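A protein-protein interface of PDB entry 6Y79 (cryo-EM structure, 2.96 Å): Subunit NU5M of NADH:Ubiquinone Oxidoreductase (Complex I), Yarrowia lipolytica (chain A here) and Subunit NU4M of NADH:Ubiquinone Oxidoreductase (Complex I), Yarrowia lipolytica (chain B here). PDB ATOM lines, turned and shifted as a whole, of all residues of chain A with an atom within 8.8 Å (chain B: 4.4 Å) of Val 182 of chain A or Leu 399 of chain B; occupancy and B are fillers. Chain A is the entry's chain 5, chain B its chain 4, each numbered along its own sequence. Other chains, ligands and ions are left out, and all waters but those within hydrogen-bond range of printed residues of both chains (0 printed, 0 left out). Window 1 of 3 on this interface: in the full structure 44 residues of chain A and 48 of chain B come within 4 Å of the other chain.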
ATOM      1  N   PHE A 140      17.257   3.699 -19.759  1.00  0.00           N
ATOM      2  CA  PHE A 140      17.662   5.055 -19.391  1.00  0.00           C
ATOM      3  C   PHE A 140      18.582   5.060 -18.174  1.00  0.00           C
ATOM      4  O   PHE A 140      19.517   5.863 -18.112  1.00  0.00           O
ATOM      5  CB  PHE A 140      16.434   5.927 -19.120  1.00  0.00           C
ATOM      6  CG  PHE A 140      16.770   7.337 -18.717  1.00  0.00           C
ATOM      7  CD1 PHE A 140      17.015   8.281 -19.674  1.00  0.00           C
ATOM      8  CD2 PHE A 140      16.833   7.718 -17.388  1.00  0.00           C
ATOM      9  CE1 PHE A 140      17.315   9.560 -19.346  1.00  0.00           C
ATOM     10  CE2 PHE A 140      17.175   8.991 -17.053  1.00  0.00           C
ATOM     11  CZ  PHE A 140      17.389   9.925 -18.037  1.00  0.00           C
ATOM     12  N   TRP A 143      21.886   3.943 -19.143  1.00  0.00           N
ATOM     13  CA  TRP A 143      22.354   4.928 -20.106  1.00  0.00           C
ATOM     14  C   TRP A 143      22.932   6.162 -19.425  1.00  0.00           C
ATOM     15  O   TRP A 143      23.905   6.747 -19.908  1.00  0.00           O
ATOM     16  CB  TRP A 143      21.172   5.285 -21.000  1.00  0.00           C
ATOM     17  CG  TRP A 143      21.433   6.210 -22.088  1.00  0.00           C
ATOM     18  CD1 TRP A 143      21.361   7.552 -22.035  1.00  0.00           C
ATOM     19  CD2 TRP A 143      21.749   5.874 -23.435  1.00  0.00           C
ATOM     20  NE1 TRP A 143      21.645   8.094 -23.257  1.00  0.00           N
ATOM     21  CE2 TRP A 143      21.882   7.078 -24.140  1.00  0.00           C
ATOM     22  CE3 TRP A 143      21.946   4.671 -24.112  1.00  0.00           C
ATOM     23  CZ2 TRP A 143      22.208   7.116 -25.484  1.00  0.00           C
ATOM     24  CZ3 TRP A 143      22.264   4.713 -25.444  1.00  0.00           C
ATOM     25  CH2 TRP A 143      22.396   5.925 -26.117  1.00  0.00           C
ATOM     26  N   GLU A 144      22.349   6.572 -18.304  1.00  0.00           N
ATOM     27  CA  GLU A 144      22.890   7.713 -17.574  1.00  0.00           C
ATOM     28  C   GLU A 144      24.078   7.342 -16.719  1.00  0.00           C
ATOM     29  O   GLU A 144      25.024   8.131 -16.582  1.00  0.00           O
ATOM     30  CB  GLU A 144      21.840   8.308 -16.668  1.00  0.00           C
ATOM     31  CG  GLU A 144      20.696   8.761 -17.405  1.00  0.00           C
ATOM     32  CD  GLU A 144      20.953  10.015 -18.128  1.00  0.00           C
ATOM     33  OE1 GLU A 144      21.719  10.865 -17.639  1.00  0.00           O
ATOM     34  OE2 GLU A 144      20.372  10.126 -19.202  1.00  0.00           O
ATOM     35  N   ASN A 174      27.218  13.814 -23.850  1.00  0.00           N
ATOM     36  CA  ASN A 174      26.298  12.733 -23.537  1.00  0.00           C
ATOM     37  C   ASN A 174      25.009  13.263 -22.926  1.00  0.00           C
ATOM     38  O   ASN A 174      23.940  12.754 -23.242  1.00  0.00           O
ATOM     39  CB  ASN A 174      26.985  11.727 -22.616  1.00  0.00           C
ATOM     40  CG  ASN A 174      28.145  11.025 -23.289  1.00  0.00           C
ATOM     41  OD1 ASN A 174      28.080  10.694 -24.470  1.00  0.00           O
ATOM     42  ND2 ASN A 174      29.219  10.811 -22.547  1.00  0.00           N
ATOM     43  N   ARG A 175      25.085  14.348 -22.150  1.00  0.00           N
ATOM     44  CA  ARG A 175      23.910  14.946 -21.530  1.00  0.00           C
ATOM     45  C   ARG A 175      23.010  15.647 -22.542  1.00  0.00           C
ATOM     46  O   ARG A 175      21.785  15.670 -22.360  1.00  0.00           O
ATOM     47  CB  ARG A 175      24.382  15.900 -20.444  1.00  0.00           C
ATOM     48  CG  ARG A 175      23.298  16.595 -19.719  1.00  0.00           C
ATOM     49  CD  ARG A 175      22.471  15.614 -18.929  1.00  0.00           C
ATOM     50  NE  ARG A 175      23.278  14.752 -18.077  1.00  0.00           N
ATOM     51  CZ  ARG A 175      22.765  13.841 -17.261  1.00  0.00           C
ATOM     52  NH1 ARG A 175      23.559  13.089 -16.516  1.00  0.00           N
ATOM     53  NH2 ARG A 175      21.453  13.684 -17.189  1.00  0.00           N
ATOM     54  N   PHE A 176      23.597  16.230 -23.593  1.00  0.00           N
ATOM     55  CA  PHE A 176      22.832  16.670 -24.758  1.00  0.00           C
ATOM     56  C   PHE A 176      21.976  15.528 -25.307  1.00  0.00           C
ATOM     57  O   PHE A 176      20.737  15.639 -25.423  1.00  0.00           O
ATOM     58  CB  PHE A 176      23.820  17.206 -25.798  1.00  0.00           C
ATOM     59  CG  PHE A 176      23.202  17.718 -27.070  1.00  0.00           C
ATOM     60  CD1 PHE A 176      22.817  19.036 -27.180  1.00  0.00           C
ATOM     61  CD2 PHE A 176      23.116  16.909 -28.191  1.00  0.00           C
ATOM     62  CE1 PHE A 176      22.290  19.529 -28.349  1.00  0.00           C
ATOM     63  CE2 PHE A 176      22.591  17.392 -29.369  1.00  0.00           C
ATOM     64  CZ  PHE A 176      22.186  18.709 -29.451  1.00  0.00           C
ATOM     65  N   GLY A 177      22.623  14.389 -25.568  1.00  0.00           N
ATOM     66  CA  GLY A 177      21.878  13.221 -26.025  1.00  0.00           C
ATOM     67  C   GLY A 177      20.864  12.692 -25.025  1.00  0.00           C
ATOM     68  O   GLY A 177      19.805  12.195 -25.413  1.00  0.00           O
ATOM     69  N   ASP A 178      21.156  12.830 -23.731  1.00  0.00           N
ATOM     70  CA  ASP A 178      20.232  12.400 -22.682  1.00  0.00           C
ATOM     71  C   ASP A 178      18.988  13.266 -22.624  1.00  0.00           C
ATOM     72  O   ASP A 178      17.903  12.767 -22.319  1.00  0.00           O
ATOM     73  CB  ASP A 178      20.910  12.401 -21.314  1.00  0.00           C
ATOM     74  CG  ASP A 178      22.119  11.499 -21.261  1.00  0.00           C
ATOM     75  OD1 ASP A 178      22.078  10.479 -21.958  1.00  0.00           O
ATOM     76  OD2 ASP A 178      23.137  11.841 -20.627  1.00  0.00           O
ATOM     77  N   ALA A 179      19.136  14.567 -22.873  1.00  0.00           N
ATOM     78  CA  ALA A 179      17.978  15.450 -22.958  1.00  0.00           C
ATOM     79  C   ALA A 179      17.065  15.051 -24.107  1.00  0.00           C
ATOM     80  O   ALA A 179      15.831  15.022 -23.959  1.00  0.00           O
ATOM     81  CB  ALA A 179      18.435  16.892 -23.128  1.00  0.00           C
ATOM     82  N   PHE A 180      17.655  14.702 -25.254  1.00  0.00           N
ATOM     83  CA  PHE A 180      16.797  14.251 -26.353  1.00  0.00           C
ATOM     84  C   PHE A 180      16.182  12.881 -26.080  1.00  0.00           C
ATOM     85  O   PHE A 180      15.055  12.609 -26.520  1.00  0.00           O
ATOM     86  CB  PHE A 180      17.562  14.263 -27.665  1.00  0.00           C
ATOM     87  CG  PHE A 180      17.787  15.638 -28.191  1.00  0.00           C
ATOM     88  CD1 PHE A 180      16.829  16.269 -28.962  1.00  0.00           C
ATOM     89  CD2 PHE A 180      18.937  16.320 -27.873  1.00  0.00           C
ATOM     90  CE1 PHE A 180      17.041  17.551 -29.427  1.00  0.00           C
ATOM     91  CE2 PHE A 180      19.149  17.591 -28.321  1.00  0.00           C
ATOM     92  CZ  PHE A 180      18.207  18.209 -29.103  1.00  0.00           C
ATOM     93  N   PHE A 181      16.860  12.030 -25.313  1.00  0.00           N
ATOM     94  CA  PHE A 181      16.237  10.764 -24.946  1.00  0.00           C
ATOM     95  C   PHE A 181      15.124  10.946 -23.920  1.00  0.00           C
ATOM     96  O   PHE A 181      14.164  10.177 -23.925  1.00  0.00           O
ATOM     97  CB  PHE A 181      17.273   9.777 -24.421  1.00  0.00           C
ATOM     98  CG  PHE A 181      16.732   8.400 -24.219  1.00  0.00           C
ATOM     99  CD1 PHE A 181      16.386   7.602 -25.288  1.00  0.00           C
ATOM    100  CD2 PHE A 181      16.547   7.912 -22.958  1.00  0.00           C
ATOM    101  CE1 PHE A 181      15.871   6.332 -25.077  1.00  0.00           C
ATOM    102  CE2 PHE A 181      16.042   6.654 -22.740  1.00  0.00           C
ATOM    103  CZ  PHE A 181      15.704   5.863 -23.798  1.00  0.00           C
ATOM    104  N   VAL A 182      15.221  11.951 -23.047  1.00  0.00           N
ATOM    105  CA  VAL A 182      14.124  12.249 -22.126  1.00  0.00           C
ATOM    106  C   VAL A 182      12.907  12.755 -22.896  1.00  0.00           C
ATOM    107  O   VAL A 182      11.766  12.384 -22.586  1.00  0.00           O
ATOM    108  CB  VAL A 182      14.592  13.243 -21.043  1.00  0.00           C
ATOM    109  CG1 VAL A 182      13.439  13.816 -20.252  1.00  0.00           C
ATOM    110  CG2 VAL A 182      15.524  12.567 -20.083  1.00  0.00           C
ATOM    111  N   LEU A 183      13.137  13.569 -23.937  1.00  0.00           N
ATOM    112  CA  LEU A 183      12.053  13.994 -24.827  1.00  0.00           C
ATOM    113  C   LEU A 183      11.376  12.805 -25.493  1.00  0.00           C
ATOM    114  O   LEU A 183      10.150  12.675 -25.441  1.00  0.00           O
ATOM    115  CB  LEU A 183      12.584  14.950 -25.893  1.00  0.00           C
ATOM    116  CG  LEU A 183      11.627  15.767 -26.772  1.00  0.00           C
ATOM    117  CD1 LEU A 183      12.261  17.098 -27.074  1.00  0.00           C
ATOM    118  CD2 LEU A 183      11.273  15.085 -28.085  1.00  0.00           C
ATOM    119  N   GLY A 184      12.162  11.925 -26.114  1.00  0.00           N
ATOM    120  CA  GLY A 184      11.586  10.762 -26.774  1.00  0.00           C
ATOM    121  C   GLY A 184      10.915   9.802 -25.810  1.00  0.00           C
ATOM    122  O   GLY A 184       9.915   9.170 -26.146  1.00  0.00           O
ATOM    123  N   LEU A 185      11.427   9.724 -24.582  1.00  0.00           N
ATOM    124  CA  LEU A 185      10.848   8.877 -23.547  1.00  0.00           C
ATOM    125  C   LEU A 185       9.501   9.413 -23.083  1.00  0.00           C
ATOM    126  O   LEU A 185       8.578   8.635 -22.804  1.00  0.00           O
ATOM    127  CB  LEU A 185      11.828   8.799 -22.381  1.00  0.00           C
ATOM    128  CG  LEU A 185      11.730   7.709 -21.331  1.00  0.00           C
ATOM    129  CD1 LEU A 185      11.772   6.407 -22.027  1.00  0.00           C
ATOM    130  CD2 LEU A 185      12.888   7.827 -20.375  1.00  0.00           C
ATOM    131  N   CYS A 186       9.378  10.740 -22.997  1.00  0.00           N
ATOM    132  CA  CYS A 186       8.094  11.359 -22.683  1.00  0.00           C
ATOM    133  C   CYS A 186       7.071  11.094 -23.779  1.00  0.00           C
ATOM    134  O   CYS A 186       5.900  10.823 -23.487  1.00  0.00           O
ATOM    135  CB  CYS A 186       8.266  12.861 -22.470  1.00  0.00           C
ATOM    136  SG  CYS A 186       9.064  13.318 -20.933  1.00  0.00           S
ATOM    137  N   VAL A 187       7.501  11.126 -25.043  1.00  0.00           N
ATOM    138  CA  VAL A 187       6.535  10.833 -26.102  1.00  0.00           C
ATOM    139  C   VAL A 187       6.177   9.342 -26.121  1.00  0.00           C
ATOM    140  O   VAL A 187       5.039   8.986 -26.441  1.00  0.00           O
ATOM    141  CB  VAL A 187       7.054  11.309 -27.473  1.00  0.00           C
ATOM    142  CG1 VAL A 187       5.935  11.301 -28.526  1.00  0.00           C
ATOM    143  CG2 VAL A 187       7.687  12.669 -27.373  1.00  0.00           C
ATOM    144  N   ILE A 188       7.125   8.460 -25.771  1.00  0.00           N
ATOM    145  CA  ILE A 188       6.849   7.023 -25.661  1.00  0.00           C
ATOM    146  C   ILE A 188       5.778   6.768 -24.611  1.00  0.00           C
ATOM    147  O   ILE A 188       4.775   6.097 -24.872  1.00  0.00           O
ATOM    148  CB  ILE A 188       8.137   6.245 -25.329  1.00  0.00           C
ATOM    149  CG1 ILE A 188       9.017   6.062 -26.556  1.00  0.00           C
ATOM    150  CG2 ILE A 188       7.818   4.878 -24.744  1.00  0.00           C
ATOM    151  CD1 ILE A 188       8.424   5.161 -27.583  1.00  0.00           C
ATOM    152  N   ALA A 189       5.965   7.327 -23.414  1.00  0.00           N
ATOM    153  CA  ALA A 189       4.997   7.125 -22.347  1.00  0.00           C
ATOM    154  C   ALA A 189       3.689   7.856 -22.605  1.00  0.00           C
ATOM    155  O   ALA A 189       2.672   7.507 -22.004  1.00  0.00           O
ATOM    156  CB  ALA A 189       5.592   7.564 -21.016  1.00  0.00           C
ATOM    157  N   TYR A 190       3.689   8.855 -23.482  1.00  0.00           N
ATOM    158  CA  TYR A 190       2.434   9.481 -23.876  1.00  0.00           C
ATOM    159  C   TYR A 190       1.653   8.613 -24.855  1.00  0.00           C
ATOM    160  O   TYR A 190       0.482   8.297 -24.627  1.00  0.00           O
ATOM    161  CB  TYR A 190       2.710  10.844 -24.494  1.00  0.00           C
ATOM    162  CG  TYR A 190       1.455  11.559 -24.857  1.00  0.00           C
ATOM    163  CD1 TYR A 190       0.464  11.752 -23.920  1.00  0.00           C
ATOM    164  CD2 TYR A 190       1.251  12.042 -26.128  1.00  0.00           C
ATOM    165  CE1 TYR A 190      -0.694  12.408 -24.234  1.00  0.00           C
ATOM    166  CE2 TYR A 190       0.095  12.707 -26.445  1.00  0.00           C
ATOM    167  CZ  TYR A 190      -0.870  12.882 -25.502  1.00  0.00           C
ATOM    168  OH  TYR A 190      -2.025  13.541 -25.832  1.00  0.00           O
ATOM    169  N   ALA A 218      14.082  11.781 -31.986  1.00  0.00           N
ATOM    170  CA  ALA A 218      14.618  12.118 -30.664  1.00  0.00           C
ATOM    171  C   ALA A 218      15.534  11.017 -30.125  1.00  0.00           C
ATOM    172  O   ALA A 218      16.639  11.292 -29.623  1.00  0.00           O
ATOM    173  CB  ALA A 218      13.472  12.387 -29.694  1.00  0.00           C
ATOM    174  N   LEU A 219      15.112   9.761 -30.271  1.00  0.00           N
ATOM    175  CA  LEU A 219      15.948   8.645 -29.841  1.00  0.00           C
ATOM    176  C   LEU A 219      17.197   8.507 -30.702  1.00  0.00           C
ATOM    177  O   LEU A 219      18.243   8.076 -30.206  1.00  0.00           O
ATOM    178  CB  LEU A 219      15.144   7.344 -29.854  1.00  0.00           C
ATOM    179  CG  LEU A 219      14.514   6.925 -28.526  1.00  0.00           C
ATOM    180  CD1 LEU A 219      13.329   7.790 -28.207  1.00  0.00           C
ATOM    181  CD2 LEU A 219      14.093   5.478 -28.570  1.00  0.00           C
ATOM    182  N   ALA A 222      19.739  11.002 -29.411  1.00  0.00           N
ATOM    183  CA  ALA A 222      20.377  10.355 -28.259  1.00  0.00           C
ATOM    184  C   ALA A 222      21.459   9.357 -28.678  1.00  0.00           C
ATOM    185  O   ALA A 222      22.609   9.426 -28.214  1.00  0.00           O
ATOM    186  CB  ALA A 222      19.324   9.644 -27.423  1.00  0.00           C
ATOM    187  N   LEU A 262      20.656   1.250 -28.598  1.00  0.00           N
ATOM    188  CA  LEU A 262      19.396   1.996 -28.617  1.00  0.00           C
ATOM    189  C   LEU A 262      18.641   1.798 -29.931  1.00  0.00           C
ATOM    190  O   LEU A 262      17.448   1.465 -29.927  1.00  0.00           O
ATOM    191  CB  LEU A 262      19.661   3.478 -28.371  1.00  0.00           C
ATOM    192  CG  LEU A 262      18.449   4.392 -28.271  1.00  0.00           C
ATOM    193  CD1 LEU A 262      17.485   3.875 -27.240  1.00  0.00           C
ATOM    194  CD2 LEU A 262      18.897   5.780 -27.911  1.00  0.00           C
ATOM    195  N   PHE B 392      15.064  12.748 -10.533  1.00  0.00           N
ATOM    196  CA  PHE B 392      14.687  12.388 -11.895  1.00  0.00           C
ATOM    197  C   PHE B 392      13.238  11.948 -11.982  1.00  0.00           C
ATOM    198  O   PHE B 392      12.597  12.180 -13.005  1.00  0.00           O
ATOM    199  CB  PHE B 392      15.561  11.287 -12.501  1.00  0.00           C
ATOM    200  CG  PHE B 392      15.157  10.957 -13.913  1.00  0.00           C
ATOM    201  CD1 PHE B 392      15.296  11.913 -14.910  1.00  0.00           C
ATOM    202  CD2 PHE B 392      14.514   9.767 -14.218  1.00  0.00           C
ATOM    203  CE1 PHE B 392      14.872  11.663 -16.195  1.00  0.00           C
ATOM    204  CE2 PHE B 392      14.084   9.515 -15.506  1.00  0.00           C
ATOM    205  CZ  PHE B 392      14.250  10.473 -16.491  1.00  0.00           C
ATOM    206  N   GLU B 395      11.358  15.240 -12.118  1.00  0.00           N
ATOM    207  CA  GLU B 395      11.596  15.950 -13.370  1.00  0.00           C
ATOM    208  C   GLU B 395      10.992  15.215 -14.556  1.00  0.00           C
ATOM    209  O   GLU B 395      10.401  15.845 -15.432  1.00  0.00           O
ATOM    210  CB  GLU B 395      13.090  16.172 -13.580  1.00  0.00           C
ATOM    211  CG  GLU B 395      13.678  17.218 -12.662  1.00  0.00           C
ATOM    212  CD  GLU B 395      15.177  17.332 -12.789  1.00  0.00           C
ATOM    213  OE1 GLU B 395      15.770  16.598 -13.607  1.00  0.00           O
ATOM    214  OE2 GLU B 395      15.773  18.119 -12.031  1.00  0.00           O
ATOM    215  N   PHE B 396      11.065  13.886 -14.565  1.00  0.00           N
ATOM    216  CA  PHE B 396      10.533  13.105 -15.670  1.00  0.00           C
ATOM    217  C   PHE B 396       9.016  13.163 -15.716  1.00  0.00           C
ATOM    218  O   PHE B 396       8.432  13.381 -16.783  1.00  0.00           O
ATOM    219  CB  PHE B 396      10.998  11.660 -15.558  1.00  0.00           C
ATOM    220  CG  PHE B 396      10.494  10.794 -16.657  1.00  0.00           C
ATOM    221  CD1 PHE B 396      10.857  11.053 -17.964  1.00  0.00           C
ATOM    222  CD2 PHE B 396       9.647   9.735 -16.393  1.00  0.00           C
ATOM    223  CE1 PHE B 396      10.389  10.270 -18.992  1.00  0.00           C
ATOM    224  CE2 PHE B 396       9.174   8.947 -17.419  1.00  0.00           C
ATOM    225  CZ  PHE B 396       9.547   9.216 -18.720  1.00  0.00           C
ATOM    226  N   LEU B 397       8.353  12.999 -14.564  1.00  0.00           N
ATOM    227  CA  LEU B 397       6.897  13.014 -14.593  1.00  0.00           C
ATOM    228  C   LEU B 397       6.346  14.418 -14.812  1.00  0.00           C
ATOM    229  O   LEU B 397       5.318  14.577 -15.482  1.00  0.00           O
ATOM    230  CB  LEU B 397       6.346  12.394 -13.321  1.00  0.00           C
ATOM    231  CG  LEU B 397       6.637  10.905 -13.173  1.00  0.00           C
ATOM    232  CD1 LEU B 397       6.124  10.390 -11.851  1.00  0.00           C
ATOM    233  CD2 LEU B 397       6.030  10.133 -14.319  1.00  0.00           C
ATOM    234  N   SER B 398       7.039  15.452 -14.328  1.00  0.00           N
ATOM    235  CA  SER B 398       6.596  16.815 -14.593  1.00  0.00           C
ATOM    236  C   SER B 398       6.816  17.212 -16.047  1.00  0.00           C
ATOM    237  O   SER B 398       5.969  17.897 -16.635  1.00  0.00           O
ATOM    238  CB  SER B 398       7.315  17.780 -13.663  1.00  0.00           C
ATOM    239  OG  SER B 398       6.933  17.555 -12.329  1.00  0.00           O
ATOM    240  N   LEU B 399       7.932  16.786 -16.651  1.00  0.00           N
ATOM    241  CA  LEU B 399       8.140  17.031 -18.073  1.00  0.00           C
ATOM    242  C   LEU B 399       7.147  16.259 -18.921  1.00  0.00           C
ATOM    243  O   LEU B 399       6.727  16.748 -19.971  1.00  0.00           O
ATOM    244  CB  LEU B 399       9.563  16.664 -18.484  1.00  0.00           C
ATOM    245  CG  LEU B 399      10.718  17.602 -18.127  1.00  0.00           C
ATOM    246  CD1 LEU B 399      12.031  16.989 -18.552  1.00  0.00           C
ATOM    247  CD2 LEU B 399      10.540  18.965 -18.730  1.00  0.00           C
ATOM    248  N   GLN B 400       6.724  15.080 -18.466  1.00  0.00           N
ATOM    249  CA  GLN B 400       5.737  14.320 -19.221  1.00  0.00           C
ATOM    250  C   GLN B 400       4.363  14.977 -19.164  1.00  0.00           C
ATOM    251  O   GLN B 400       3.677  15.079 -20.189  1.00  0.00           O
ATOM    252  CB  GLN B 400       5.667  12.892 -18.704  1.00  0.00           C
ATOM    253  CG  GLN B 400       4.871  12.009 -19.614  1.00  0.00           C
ATOM    254  CD  GLN B 400       4.717  10.628 -19.073  1.00  0.00           C
ATOM    255  OE1 GLN B 400       5.473  10.201 -18.201  1.00  0.00           O
ATOM    256  NE2 GLN B 400       3.713   9.917 -19.563  1.00  0.00           N
ATOM    257  N   GLY B 401       3.942  15.425 -17.975  1.00  0.00           N
ATOM    258  CA  GLY B 401       2.689  16.161 -17.869  1.00  0.00           C
ATOM    259  C   GLY B 401       2.693  17.458 -18.658  1.00  0.00           C
ATOM    260  O   GLY B 401       1.719  17.780 -19.352  1.00  0.00           O
ATOM    261  N   GLY B 402       3.798  18.203 -18.594  1.00  0.00           N
ATOM    262  CA  GLY B 402       3.946  19.383 -19.420  1.00  0.00           C
ATOM    263  C   GLY B 402       4.027  19.096 -20.902  1.00  0.00           C
ATOM    264  O   GLY B 402       3.732  19.979 -21.707  1.00  0.00           O
ATOM    265  N   PHE B 403       4.430  17.886 -21.286  1.00  0.00           N
ATOM    266  CA  PHE B 403       4.337  17.515 -22.689  1.00  0.00           C
ATOM    267  C   PHE B 403       2.910  17.186 -23.096  1.00  0.00           C
ATOM    268  O   PHE B 403       2.544  17.399 -24.255  1.00  0.00           O
ATOM    269  CB  PHE B 403       5.244  16.325 -22.997  1.00  0.00           C
ATOM    270  CG  PHE B 403       5.253  15.949 -24.446  1.00  0.00           C
ATOM    271  CD1 PHE B 403       5.947  16.716 -25.355  1.00  0.00           C
ATOM    272  CD2 PHE B 403       4.532  14.858 -24.904  1.00  0.00           C
ATOM    273  CE1 PHE B 403       5.947  16.398 -26.689  1.00  0.00           C
ATOM    274  CE2 PHE B 403       4.519  14.535 -26.241  1.00  0.00           C
ATOM    275  CZ  PHE B 403       5.234  15.306 -27.133  1.00  0.00           C
ATOM    276  N   SER B 413      10.986  22.505 -23.002  1.00  0.00           N
ATOM    277  CA  SER B 413      11.257  22.363 -21.578  1.00  0.00           C
ATOM    278  C   SER B 413      12.091  21.136 -21.266  1.00  0.00           C
ATOM    279  O   SER B 413      12.688  21.075 -20.191  1.00  0.00           O
ATOM    280  CB  SER B 413       9.944  22.317 -20.783  1.00  0.00           C
ATOM    281  OG  SER B 413       9.328  23.591 -20.763  1.00  0.00           O
ATOM    282  N   CYS B 414      12.153  20.167 -22.185  1.00  0.00           N
ATOM    283  CA  CYS B 414      12.973  18.979 -21.974  1.00  0.00           C
ATOM    284  C   CYS B 414      14.476  19.251 -21.996  1.00  0.00           C
ATOM    285  O   CYS B 414      15.236  18.411 -21.510  1.00  0.00           O
ATOM    286  CB  CYS B 414      12.625  17.918 -23.016  1.00  0.00           C
ATOM    287  SG  CYS B 414      11.218  16.880 -22.561  1.00  0.00           S
ATOM    288  N   VAL B 417      17.187  19.193 -18.758  1.00  0.00           N
ATOM    289  CA  VAL B 417      18.090  18.096 -18.415  1.00  0.00           C
ATOM    290  C   VAL B 417      19.531  18.451 -18.768  1.00  0.00           C
ATOM    291  O   VAL B 417      20.462  18.190 -17.997  1.00  0.00           O
ATOM    292  CB  VAL B 417      17.627  16.815 -19.133  1.00  0.00           C
ATOM    293  CG1 VAL B 417      18.622  15.688 -18.967  1.00  0.00           C
ATOM    294  CG2 VAL B 417      16.268  16.399 -18.626  1.00  0.00           C
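The guanidinium group of Arg 175 of chain A lies within salt-bridge range of the side-chain carboxylate of Glu 144 of chain A.
O of Val 182 of chain A is in hydrogen-bond range of SG of Cys 186 of chain A, 3.3 Å away.
OD2 of Asp 178 of chain A is in salt-bridge range of NE of Arg 175 of chain A (3.9 Å).
Phe 140 of chain A touches Phe 392 of chain B (CE2 to CZ, 3.3 Å).
Val 417 of chain B touches Arg 175 of chain A (O to CD, 3.4 Å).
Ala 179 of chain A touches Cys 414 of chain B (CB to O, 3.9 Å).
CG1 of Val 182 of chain A touches CD1 of Leu 399 of chain B (3.9 Å).
CA of Leu 183 of chain A touches SG of Cys 414 of chain B, 3.8 Å away.
Phe 396 of chain B touches Leu 185 of chain A (CE1 to CG, 3.7 Å).
Cys 186 of chain A touches Phe 396 of chain B.
Gln 400 of chain B touches Cys 186 of chain A.
Val 187 of chain A touches Phe 403 of chain B (CG2 to CZ, 3.6 Å).
Ala 189 of chain A touches Gln 400 of chain B.
Trp 143 of chain A touches none of the printed residues of chain B.
Printed residues of chain B within 4 Å of Arg 175 of chain A: Val 417 (3.4 Å).
Val 182 of chain A touches just one residue of chain B: Leu 399 (3.9 Å).
Of the printed residues of chain B, Cys 186 of chain A touches Phe 396 (3.8 Å) and Gln 400 (3.8 Å).
Of the printed residues of chain B, Ala 189 of chain A touches Gln 400.
Printed residues of chain A within 4 Å of Phe 392 of chain B: Phe 140 (3.3 Å).
No residue of chain A comes within 4 Å of Ser 398 of chain B.
Leu 399 of chain B touches just one residue of chain A: Val 182.
The nearest residue of chain B that does not touch Val 182 of chain A is Phe 392 of chain B (4.04 Å).
The nearest residue of chain A that does not touch Leu 399 of chain B is Cys 186 of chain A (4.05 Å).
Printed residues of chain A that touch a printed residue of chain B: Phe 140, Arg 175, Ala 179, Val 182, Leu 183, Leu 185, Cys 186, Val 187 and Ala 189.
Hydrophobic or aromatic side chains of chain A within 4 Å of the printed part of chain B: Phe 140, Ala 179, Val 182, Leu 185, Val 187 and Ala 189.
Along chain A the printed residues that touch a printed residue of chain B span positions 140 to 189.
Of the 13 printed residues of chain B, 7 touch a printed residue of chain A.
Among the printed residues, 10 pairs touch across the chains.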
